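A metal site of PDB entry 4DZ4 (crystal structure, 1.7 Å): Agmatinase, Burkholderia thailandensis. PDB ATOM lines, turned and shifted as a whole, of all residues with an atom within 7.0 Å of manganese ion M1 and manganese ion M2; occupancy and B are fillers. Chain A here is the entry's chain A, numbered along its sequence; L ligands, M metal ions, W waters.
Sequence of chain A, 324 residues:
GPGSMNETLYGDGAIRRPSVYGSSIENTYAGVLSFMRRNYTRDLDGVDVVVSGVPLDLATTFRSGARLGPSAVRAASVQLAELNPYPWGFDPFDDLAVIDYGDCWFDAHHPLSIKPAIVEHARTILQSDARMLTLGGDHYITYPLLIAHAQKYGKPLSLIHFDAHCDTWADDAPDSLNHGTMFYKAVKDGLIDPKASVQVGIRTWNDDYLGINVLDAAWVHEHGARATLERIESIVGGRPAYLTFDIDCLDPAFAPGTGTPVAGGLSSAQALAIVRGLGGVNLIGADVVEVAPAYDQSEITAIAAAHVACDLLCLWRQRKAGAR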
ATOM      1  N   ASP A 138      -5.737 -18.000  -1.754  1.00  0.00           N
ATOM      2  CA  ASP A 138      -5.575 -16.653  -1.213  1.00  0.00           C
ATOM      3  C   ASP A 138      -6.776 -16.215  -0.397  1.00  0.00           C
ATOM      4  O   ASP A 138      -7.826 -16.893  -0.378  1.00  0.00           O
ATOM      5  CB  ASP A 138      -5.176 -15.630  -2.298  1.00  0.00           C
ATOM      6  CG  ASP A 138      -6.332 -15.247  -3.251  1.00  0.00           C
ATOM      7  OD1 ASP A 138      -7.464 -14.974  -2.782  1.00  0.00           O
ATOM      8  OD2 ASP A 138      -6.095 -15.183  -4.489  1.00  0.00           O
ATOM      9  N   HIS A 139      -6.612 -15.113   0.340  1.00  0.00           N
ATOM     10  CA  HIS A 139      -7.600 -14.742   1.348  1.00  0.00           C
ATOM     11  C   HIS A 139      -8.920 -14.351   0.764  1.00  0.00           C
ATOM     12  O   HIS A 139      -9.932 -14.279   1.485  1.00  0.00           O
ATOM     13  CB  HIS A 139      -7.062 -13.651   2.253  1.00  0.00           C
ATOM     14  CG  HIS A 139      -7.467 -13.812   3.697  1.00  0.00           C
ATOM     15  ND1 HIS A 139      -6.802 -13.214   4.714  1.00  0.00           N
ATOM     16  CD2 HIS A 139      -8.494 -14.539   4.265  1.00  0.00           C
ATOM     17  CE1 HIS A 139      -7.363 -13.564   5.873  1.00  0.00           C
ATOM     18  NE2 HIS A 139      -8.409 -14.384   5.603  1.00  0.00           N
ATOM     19  N   TYR A 140      -8.967 -14.065  -0.529  1.00  0.00           N
ATOM     20  CA  TYR A 140     -10.230 -13.631  -1.122  1.00  0.00           C
ATOM     21  C   TYR A 140     -11.288 -14.731  -0.917  1.00  0.00           C
ATOM     22  O   TYR A 140     -12.486 -14.434  -0.770  1.00  0.00           O
ATOM     23  CB  TYR A 140     -10.098 -13.258  -2.604  1.00  0.00           C
ATOM     24  CG  TYR A 140     -11.463 -12.956  -3.244  1.00  0.00           C
ATOM     25  CD1 TYR A 140     -12.033 -11.685  -3.162  1.00  0.00           C
ATOM     26  CD2 TYR A 140     -12.205 -13.975  -3.867  1.00  0.00           C
ATOM     27  CE1 TYR A 140     -13.282 -11.426  -3.735  1.00  0.00           C
ATOM     28  CE2 TYR A 140     -13.470 -13.735  -4.421  1.00  0.00           C
ATOM     29  CZ  TYR A 140     -14.007 -12.451  -4.350  1.00  0.00           C
ATOM     30  OH  TYR A 140     -15.261 -12.195  -4.915  1.00  0.00           O
ATOM     31  N   HIS A 161      -9.970 -13.159  12.971  1.00  0.00           N
ATOM     32  CA  HIS A 161      -9.122 -13.031  11.781  1.00  0.00           C
ATOM     33  C   HIS A 161      -7.675 -12.899  12.211  1.00  0.00           C
ATOM     34  O   HIS A 161      -7.312 -11.911  12.871  1.00  0.00           O
ATOM     35  CB  HIS A 161      -9.678 -11.816  11.011  1.00  0.00           C
ATOM     36  CG  HIS A 161      -8.877 -11.370   9.820  1.00  0.00           C
ATOM     37  ND1 HIS A 161      -8.990 -10.099   9.331  1.00  0.00           N
ATOM     38  CD2 HIS A 161      -7.943 -12.018   9.020  1.00  0.00           C
ATOM     39  CE1 HIS A 161      -8.192  -9.953   8.269  1.00  0.00           C
ATOM     40  NE2 HIS A 161      -7.558 -11.127   8.055  1.00  0.00           N
ATOM     41  N   PHE A 162      -6.864 -13.911  11.904  1.00  0.00           N
ATOM     42  CA  PHE A 162      -5.407 -13.909  12.169  1.00  0.00           C
ATOM     43  C   PHE A 162      -4.695 -13.509  10.876  1.00  0.00           C
ATOM     44  O   PHE A 162      -4.904 -14.148   9.850  1.00  0.00           O
ATOM     45  CB  PHE A 162      -4.923 -15.298  12.562  1.00  0.00           C
ATOM     46  CG  PHE A 162      -5.392 -15.740  13.927  1.00  0.00           C
ATOM     47  CD1 PHE A 162      -6.643 -16.340  14.069  1.00  0.00           C
ATOM     48  CD2 PHE A 162      -4.581 -15.590  15.051  1.00  0.00           C
ATOM     49  CE1 PHE A 162      -7.076 -16.753  15.330  1.00  0.00           C
ATOM     50  CE2 PHE A 162      -5.014 -15.995  16.317  1.00  0.00           C
ATOM     51  CZ  PHE A 162      -6.275 -16.608  16.446  1.00  0.00           C
ATOM     52  N   ASP A 163      -3.859 -12.451  10.916  1.00  0.00           N
ATOM     53  CA  ASP A 163      -3.337 -11.872   9.684  1.00  0.00           C
ATOM     54  C   ASP A 163      -2.373 -10.748   9.988  1.00  0.00           C
ATOM     55  O   ASP A 163      -2.525 -10.042  10.993  1.00  0.00           O
ATOM     56  CB  ASP A 163      -4.526 -11.321   8.875  1.00  0.00           C
ATOM     57  CG  ASP A 163      -4.299 -11.319   7.374  1.00  0.00           C
ATOM     58  OD1 ASP A 163      -3.177 -11.021   6.915  1.00  0.00           O
ATOM     59  OD2 ASP A 163      -5.263 -11.570   6.627  1.00  0.00           O
ATOM     60  N   ALA A 164      -1.376 -10.546   9.128  1.00  0.00           N
ATOM     61  CA  ALA A 164      -0.589  -9.300   9.235  1.00  0.00           C
ATOM     62  C   ALA A 164      -1.371  -8.117   8.650  1.00  0.00           C
ATOM     63  O   ALA A 164      -1.014  -6.974   8.920  1.00  0.00           O
ATOM     64  CB  ALA A 164       0.727  -9.450   8.469  1.00  0.00           C
ATOM     65  N   HIS A 165      -2.400  -8.445   7.852  1.00  0.00           N
ATOM     66  CA  HIS A 165      -3.174  -7.474   7.063  1.00  0.00           C
ATOM     67  C   HIS A 165      -4.617  -7.466   7.494  1.00  0.00           C
ATOM     68  O   HIS A 165      -5.230  -8.522   7.684  1.00  0.00           O
ATOM     69  CB  HIS A 165      -3.156  -7.871   5.593  1.00  0.00           C
ATOM     70  CG  HIS A 165      -1.757  -8.055   5.055  1.00  0.00           C
ATOM     71  ND1 HIS A 165      -1.146  -9.261   4.990  1.00  0.00           N
ATOM     72  CD2 HIS A 165      -0.835  -7.126   4.612  1.00  0.00           C
ATOM     73  CE1 HIS A 165       0.115  -9.094   4.522  1.00  0.00           C
ATOM     74  NE2 HIS A 165       0.294  -7.790   4.270  1.00  0.00           N
ATOM     75  N   CYS A 166      -5.165  -6.258   7.600  1.00  0.00           N
ATOM     76  CA  CYS A 166      -6.566  -6.116   8.005  1.00  0.00           C
ATOM     77  C   CYS A 166      -7.554  -6.513   6.898  1.00  0.00           C
ATOM     78  O   CYS A 166      -8.706  -6.883   7.181  1.00  0.00           O
ATOM     79  CB  CYS A 166      -6.830  -4.682   8.481  1.00  0.00           C
ATOM     80  SG  CYS A 166      -6.582  -3.452   7.164  1.00  0.00           S
ATOM     81  N   ASP A 167      -7.119  -6.429   5.630  1.00  0.00           N
ATOM     82  CA  ASP A 167      -7.980  -6.729   4.457  1.00  0.00           C
ATOM     83  C   ASP A 167      -9.292  -5.945   4.459  1.00  0.00           C
ATOM     84  O   ASP A 167     -10.309  -6.408   3.924  1.00  0.00           O
ATOM     85  CB  ASP A 167      -8.213  -8.236   4.317  1.00  0.00           C
ATOM     86  CG  ASP A 167      -6.919  -8.982   4.208  1.00  0.00           C
ATOM     87  OD1 ASP A 167      -5.895  -8.373   3.775  1.00  0.00           O
ATOM     88  OD2 ASP A 167      -6.871 -10.166   4.556  1.00  0.00           O
ATOM     89  N   TRP A 169      -9.164  -2.520   3.531  1.00  0.00           N
ATOM     90  CA  TRP A 169      -8.934  -1.303   2.728  1.00  0.00           C
ATOM     91  C   TRP A 169     -10.134  -1.067   1.847  1.00  0.00           C
ATOM     92  O   TRP A 169     -10.706  -2.041   1.327  1.00  0.00           O
ATOM     93  CB  TRP A 169      -7.634  -1.436   1.935  1.00  0.00           C
ATOM     94  CG  TRP A 169      -6.441  -1.450   2.873  1.00  0.00           C
ATOM     95  CD1 TRP A 169      -5.876  -0.349   3.522  1.00  0.00           C
ATOM     96  CD2 TRP A 169      -5.657  -2.615   3.341  1.00  0.00           C
ATOM     97  NE1 TRP A 169      -4.819  -0.722   4.314  1.00  0.00           N
ATOM     98  CE2 TRP A 169      -4.635  -2.068   4.246  1.00  0.00           C
ATOM     99  CE3 TRP A 169      -5.672  -3.983   3.073  1.00  0.00           C
ATOM    100  CZ2 TRP A 169      -3.695  -2.887   4.878  1.00  0.00           C
ATOM    101  CZ3 TRP A 169      -4.721  -4.789   3.719  1.00  0.00           C
ATOM    102  CH2 TRP A 169      -3.759  -4.251   4.594  1.00  0.00           C
ATOM    103  N   HIS A 179      -7.633  -9.844  -2.539  1.00  0.00           N
ATOM    104  CA  HIS A 179      -7.516 -10.477  -1.218  1.00  0.00           C
ATOM    105  C   HIS A 179      -7.299  -9.519  -0.082  1.00  0.00           C
ATOM    106  O   HIS A 179      -7.220  -9.949   1.066  1.00  0.00           O
ATOM    107  CB  HIS A 179      -6.431 -11.580  -1.203  1.00  0.00           C
ATOM    108  CG  HIS A 179      -4.999 -11.062  -1.329  1.00  0.00           C
ATOM    109  ND1 HIS A 179      -3.920 -11.820  -0.974  1.00  0.00           N
ATOM    110  CD2 HIS A 179      -4.487  -9.850  -1.779  1.00  0.00           C
ATOM    111  CE1 HIS A 179      -2.774 -11.129  -1.192  1.00  0.00           C
ATOM    112  NE2 HIS A 179      -3.108  -9.916  -1.682  1.00  0.00           N
ATOM    113  N   GLY A 180      -7.238  -8.216  -0.384  1.00  0.00           N
ATOM    114  CA  GLY A 180      -7.005  -7.199   0.637  1.00  0.00           C
ATOM    115  C   GLY A 180      -8.163  -6.238   0.841  1.00  0.00           C
ATOM    116  O   GLY A 180      -8.091  -5.329   1.661  1.00  0.00           O
ATOM    117  N   MET A 182     -11.703  -7.605   0.772  1.00  0.00           N
ATOM    118  CA  MET A 182     -12.954  -8.360   0.883  1.00  0.00           C
ATOM    119  C   MET A 182     -13.615  -8.241   2.263  1.00  0.00           C
ATOM    120  O   MET A 182     -14.825  -8.444   2.382  1.00  0.00           O
ATOM    121  CB  MET A 182     -12.785  -9.827   0.408  1.00  0.00           C
ATOM    122  CG  MET A 182     -12.008 -10.749   1.360  1.00  0.00           C
ATOM    123  SD  MET A 182     -10.238 -10.486   1.269  1.00  0.00           S
ATOM    124  CE  MET A 182      -9.778 -11.286   2.822  1.00  0.00           C
ATOM    125  N   PHE A 183     -12.863  -7.872   3.297  1.00  0.00           N
ATOM    126  CA  PHE A 183     -13.477  -7.647   4.616  1.00  0.00           C
ATOM    127  C   PHE A 183     -14.059  -6.241   4.790  1.00  0.00           C
ATOM    128  O   PHE A 183     -14.959  -6.036   5.615  1.00  0.00           O
ATOM    129  CB  PHE A 183     -12.568  -8.052   5.782  1.00  0.00           C
ATOM    130  CG  PHE A 183     -12.207  -9.521   5.808  1.00  0.00           C
ATOM    131  CD1 PHE A 183     -13.045 -10.485   5.238  1.00  0.00           C
ATOM    132  CD2 PHE A 183     -11.023  -9.945   6.405  1.00  0.00           C
ATOM    133  CE1 PHE A 183     -12.725 -11.830   5.256  1.00  0.00           C
ATOM    134  CE2 PHE A 183     -10.694 -11.293   6.427  1.00  0.00           C
ATOM    135  CZ  PHE A 183     -11.543 -12.238   5.846  1.00  0.00           C
ATOM    136  N   THR A 244     -10.727 -17.183  10.487  1.00  0.00           N
ATOM    137  CA  THR A 244      -9.962 -17.191   9.234  1.00  0.00           C
ATOM    138  C   THR A 244      -8.513 -16.944   9.578  1.00  0.00           C
ATOM    139  O   THR A 244      -8.177 -15.957  10.246  1.00  0.00           O
ATOM    140  CB  THR A 244     -10.517 -16.173   8.212  1.00  0.00           C
ATOM    141  OG1 THR A 244      -9.708 -16.184   7.037  1.00  0.00           O
ATOM    142  CG2 THR A 244     -10.534 -14.722   8.801  1.00  0.00           C
ATOM    143  N   ASP A 246      -4.887 -16.435   8.140  1.00  0.00           N
ATOM    144  CA  ASP A 246      -3.895 -16.165   7.092  1.00  0.00           C
ATOM    145  C   ASP A 246      -2.528 -16.487   7.661  1.00  0.00           C
ATOM    146  O   ASP A 246      -2.136 -15.954   8.705  1.00  0.00           O
ATOM    147  CB  ASP A 246      -4.012 -14.688   6.667  1.00  0.00           C
ATOM    148  CG  ASP A 246      -3.027 -14.280   5.601  1.00  0.00           C
ATOM    149  OD1 ASP A 246      -2.009 -14.967   5.355  1.00  0.00           O
ATOM    150  OD2 ASP A 246      -3.292 -13.240   4.988  1.00  0.00           O
ATOM    151  N   ILE A 247      -1.807 -17.386   6.981  1.00  0.00           N
ATOM    152  CA  ILE A 247      -0.551 -17.903   7.518  1.00  0.00           C
ATOM    153  C   ILE A 247       0.485 -16.773   7.643  1.00  0.00           C
ATOM    154  O   ILE A 247       1.419 -16.883   8.450  1.00  0.00           O
ATOM    155  CB  ILE A 247      -0.007 -19.105   6.704  1.00  0.00           C
ATOM    156  CG1 ILE A 247       0.901 -20.002   7.573  1.00  0.00           C
ATOM    157  CG2 ILE A 247       0.657 -18.667   5.397  1.00  0.00           C
ATOM    158  CD1 ILE A 247       0.230 -20.637   8.800  1.00  0.00           C
ATOM    159  N   ASP A 248       0.287 -15.677   6.907  1.00  0.00           N
ATOM    160  CA  ASP A 248       1.212 -14.534   7.081  1.00  0.00           C
ATOM    161  C   ASP A 248       1.068 -13.764   8.410  1.00  0.00           C
ATOM    162  O   ASP A 248       1.809 -12.829   8.678  1.00  0.00           O
ATOM    163  CB  ASP A 248       1.229 -13.612   5.847  1.00  0.00           C
ATOM    164  CG  ASP A 248      -0.021 -12.741   5.712  1.00  0.00           C
ATOM    165  OD1 ASP A 248      -0.717 -12.468   6.735  1.00  0.00           O
ATOM    166  OD2 ASP A 248      -0.289 -12.309   4.571  1.00  0.00           O
ATOM    167  N   CYS A 249       0.110 -14.189   9.246  1.00  0.00           N
ATOM    168  CA  CYS A 249       0.074 -13.754  10.632  1.00  0.00           C
ATOM    169  C   CYS A 249       1.406 -14.095  11.310  1.00  0.00           C
ATOM    170  O   CYS A 249       1.972 -13.300  12.075  1.00  0.00           O
ATOM    171  CB  CYS A 249      -1.082 -14.469  11.340  1.00  0.00           C
ATOM    172  SG  CYS A 249      -1.181 -14.108  13.110  1.00  0.00           S
ATOM    173  N   THR A 258       4.643 -17.620   1.707  1.00  0.00           N
ATOM    174  CA  THR A 258       3.406 -16.841   1.590  1.00  0.00           C
ATOM    175  C   THR A 258       3.621 -15.688   0.636  1.00  0.00           C
ATOM    176  O   THR A 258       4.773 -15.289   0.405  1.00  0.00           O
ATOM    177  CB  THR A 258       2.938 -16.428   3.010  1.00  0.00           C
ATOM    178  OG1 THR A 258       1.528 -16.087   2.966  1.00  0.00           O
ATOM    179  CG2 THR A 258       3.801 -15.290   3.548  1.00  0.00           C
ATOM    180  N   THR A 260       2.624 -12.360   0.686  1.00  0.00           N
ATOM    181  CA  THR A 260       2.831 -10.986   1.204  1.00  0.00           C
ATOM    182  C   THR A 260       3.467 -11.050   2.603  1.00  0.00           C
ATOM    183  O   THR A 260       2.812 -10.778   3.614  1.00  0.00           O
ATOM    184  CB  THR A 260       1.502 -10.165   1.249  1.00  0.00           C
ATOM    185  OG1 THR A 260       0.467 -10.973   1.840  1.00  0.00           O
ATOM    186  CG2 THR A 260       1.069  -9.707  -0.148  1.00  0.00           C
ATOM    187  N   VAL A 262       5.453 -10.072   5.930  1.00  0.00           N
ATOM    188  CA  VAL A 262       5.672  -8.813   6.658  1.00  0.00           C
ATOM    189  C   VAL A 262       6.446  -9.100   7.943  1.00  0.00           C
ATOM    190  O   VAL A 262       6.033  -9.931   8.740  1.00  0.00           O
ATOM    191  CB  VAL A 262       4.327  -8.143   7.069  1.00  0.00           C
ATOM    192  CG1 VAL A 262       4.617  -6.794   7.717  1.00  0.00           C
ATOM    193  CG2 VAL A 262       3.385  -8.012   5.886  1.00  0.00           C
ATOM    194  N   VAL A 289      -5.413 -19.979   5.132  1.00  0.00           N
ATOM    195  CA  VAL A 289      -5.197 -19.451   3.784  1.00  0.00           C
ATOM    196  C   VAL A 289      -3.782 -18.921   3.576  1.00  0.00           C
ATOM    197  O   VAL A 289      -3.032 -18.723   4.544  1.00  0.00           O
ATOM    198  CB  VAL A 289      -6.209 -18.330   3.418  1.00  0.00           C
ATOM    199  CG1 VAL A 289      -7.647 -18.858   3.524  1.00  0.00           C
ATOM    200  CG2 VAL A 289      -6.037 -17.122   4.359  1.00  0.00           C
ATOM    201  N   GLU A 290      -3.478 -18.716   2.290  1.00  0.00           N
ATOM    202  CA  GLU A 290      -2.260 -18.013   1.820  1.00  0.00           C
ATOM    203  C   GLU A 290      -0.963 -18.844   1.888  1.00  0.00           C
ATOM    204  O   GLU A 290       0.131 -18.286   1.718  1.00  0.00           O
ATOM    205  CB  GLU A 290      -2.068 -16.625   2.487  1.00  0.00           C
ATOM    206  CG  GLU A 290      -3.158 -15.583   2.226  1.00  0.00           C
ATOM    207  CD  GLU A 290      -3.069 -14.928   0.829  1.00  0.00           C
ATOM    208  OE1 GLU A 290      -2.080 -15.153   0.102  1.00  0.00           O
ATOM    209  OE2 GLU A 290      -3.973 -14.147   0.468  1.00  0.00           O
HETATM  210  O1  LIG L   1      -2.409 -11.295   2.179  1.00  0.00           O
HETATM  211  O1  LG2 L   2      -5.184 -11.235   2.271  1.00  0.00           O
HETATM  212 MN    MN M   1      -2.149 -11.336   5.096  1.00  0.00          MN
HETATM  213 MN    MN M   2      -5.331 -11.576   4.481  1.00  0.00          MN
HETATM  214  O   HOH W   1      -3.737 -10.595   3.942  1.00  0.00           O
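The backbone carbonyl oxygen (O) of Asp 167 is in hydrogen-bond range of the backbone NH (N) of Phe 183. A ring nitrogen (NE2) of His 161 lies close to the side-chain carboxylate of Asp 163, at 2.7 Å. The side-chain carboxylate (OD1) of Asp 248 sits close to the backbone NH (N) of Ala 164. OD2 of Asp 248 sits close to OG1 of Thr 260, 3.1 Å away. N of His 139 is in hydrogen-bond range of OE2 of Glu 290, 2.8 Å away. OG1 of Thr 244 is in hydrogen-bond range of NE2 of His 139 (2.6 Å). The backbone NH of Asp 246 sits at hydrogen-bond distance from the backbone carbonyl oxygen of Phe 162 (2.9 Å).
Four residues have an atom within 4 Å of manganese ion M1: Asp 163, His 165, Asp 246 and Asp 248. The nearest printed residue that does not touch manganese ion M1 is Ala 164 (4.2 Å).
The nearest printed residue that does not touch manganese ion M2 is His 179 (4.2 Å).
Water W1 binds manganese ion M1, 2.1 Å away. The side-chain carboxylate (OD1) of Asp 163 is bound to manganese ion M1 (2.1 Å). The side-chain carboxylate (OD2) of Asp 248 binds manganese ion M1 (2.2 Å). The side-chain carboxylate (OD2) of Asp 246 binds manganese ion M1. ND1 of His 165 binds manganese ion M1, 2.3 Å away. Manganese ion M1 is bound by the side-chain carboxylate (OD1) of Asp 248 (2.5 Å). Manganese ion M1 has six donor atoms within binding distance. Slightly farther from manganese ion M1 lies O1 of LIG L1 (2.9 Å).
Manganese ion M2 is bound by water W1. Manganese ion M2 is bound by the side-chain carboxylate (OD2) of Asp 167, at 2.1 Å. Manganese ion M2 is bound by OD2 of Asp 163 (2.1 Å). Manganese ion M2 is bound by a ring nitrogen (ND1) of His 139 (2.2 Å). O1 of LG2 L2 is bound to manganese ion M2 (2.2 Å). OD2 of Asp 246 is bound to manganese ion M2, 2.7 Å away. Manganese ion M2 has six donor atoms within binding distance.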
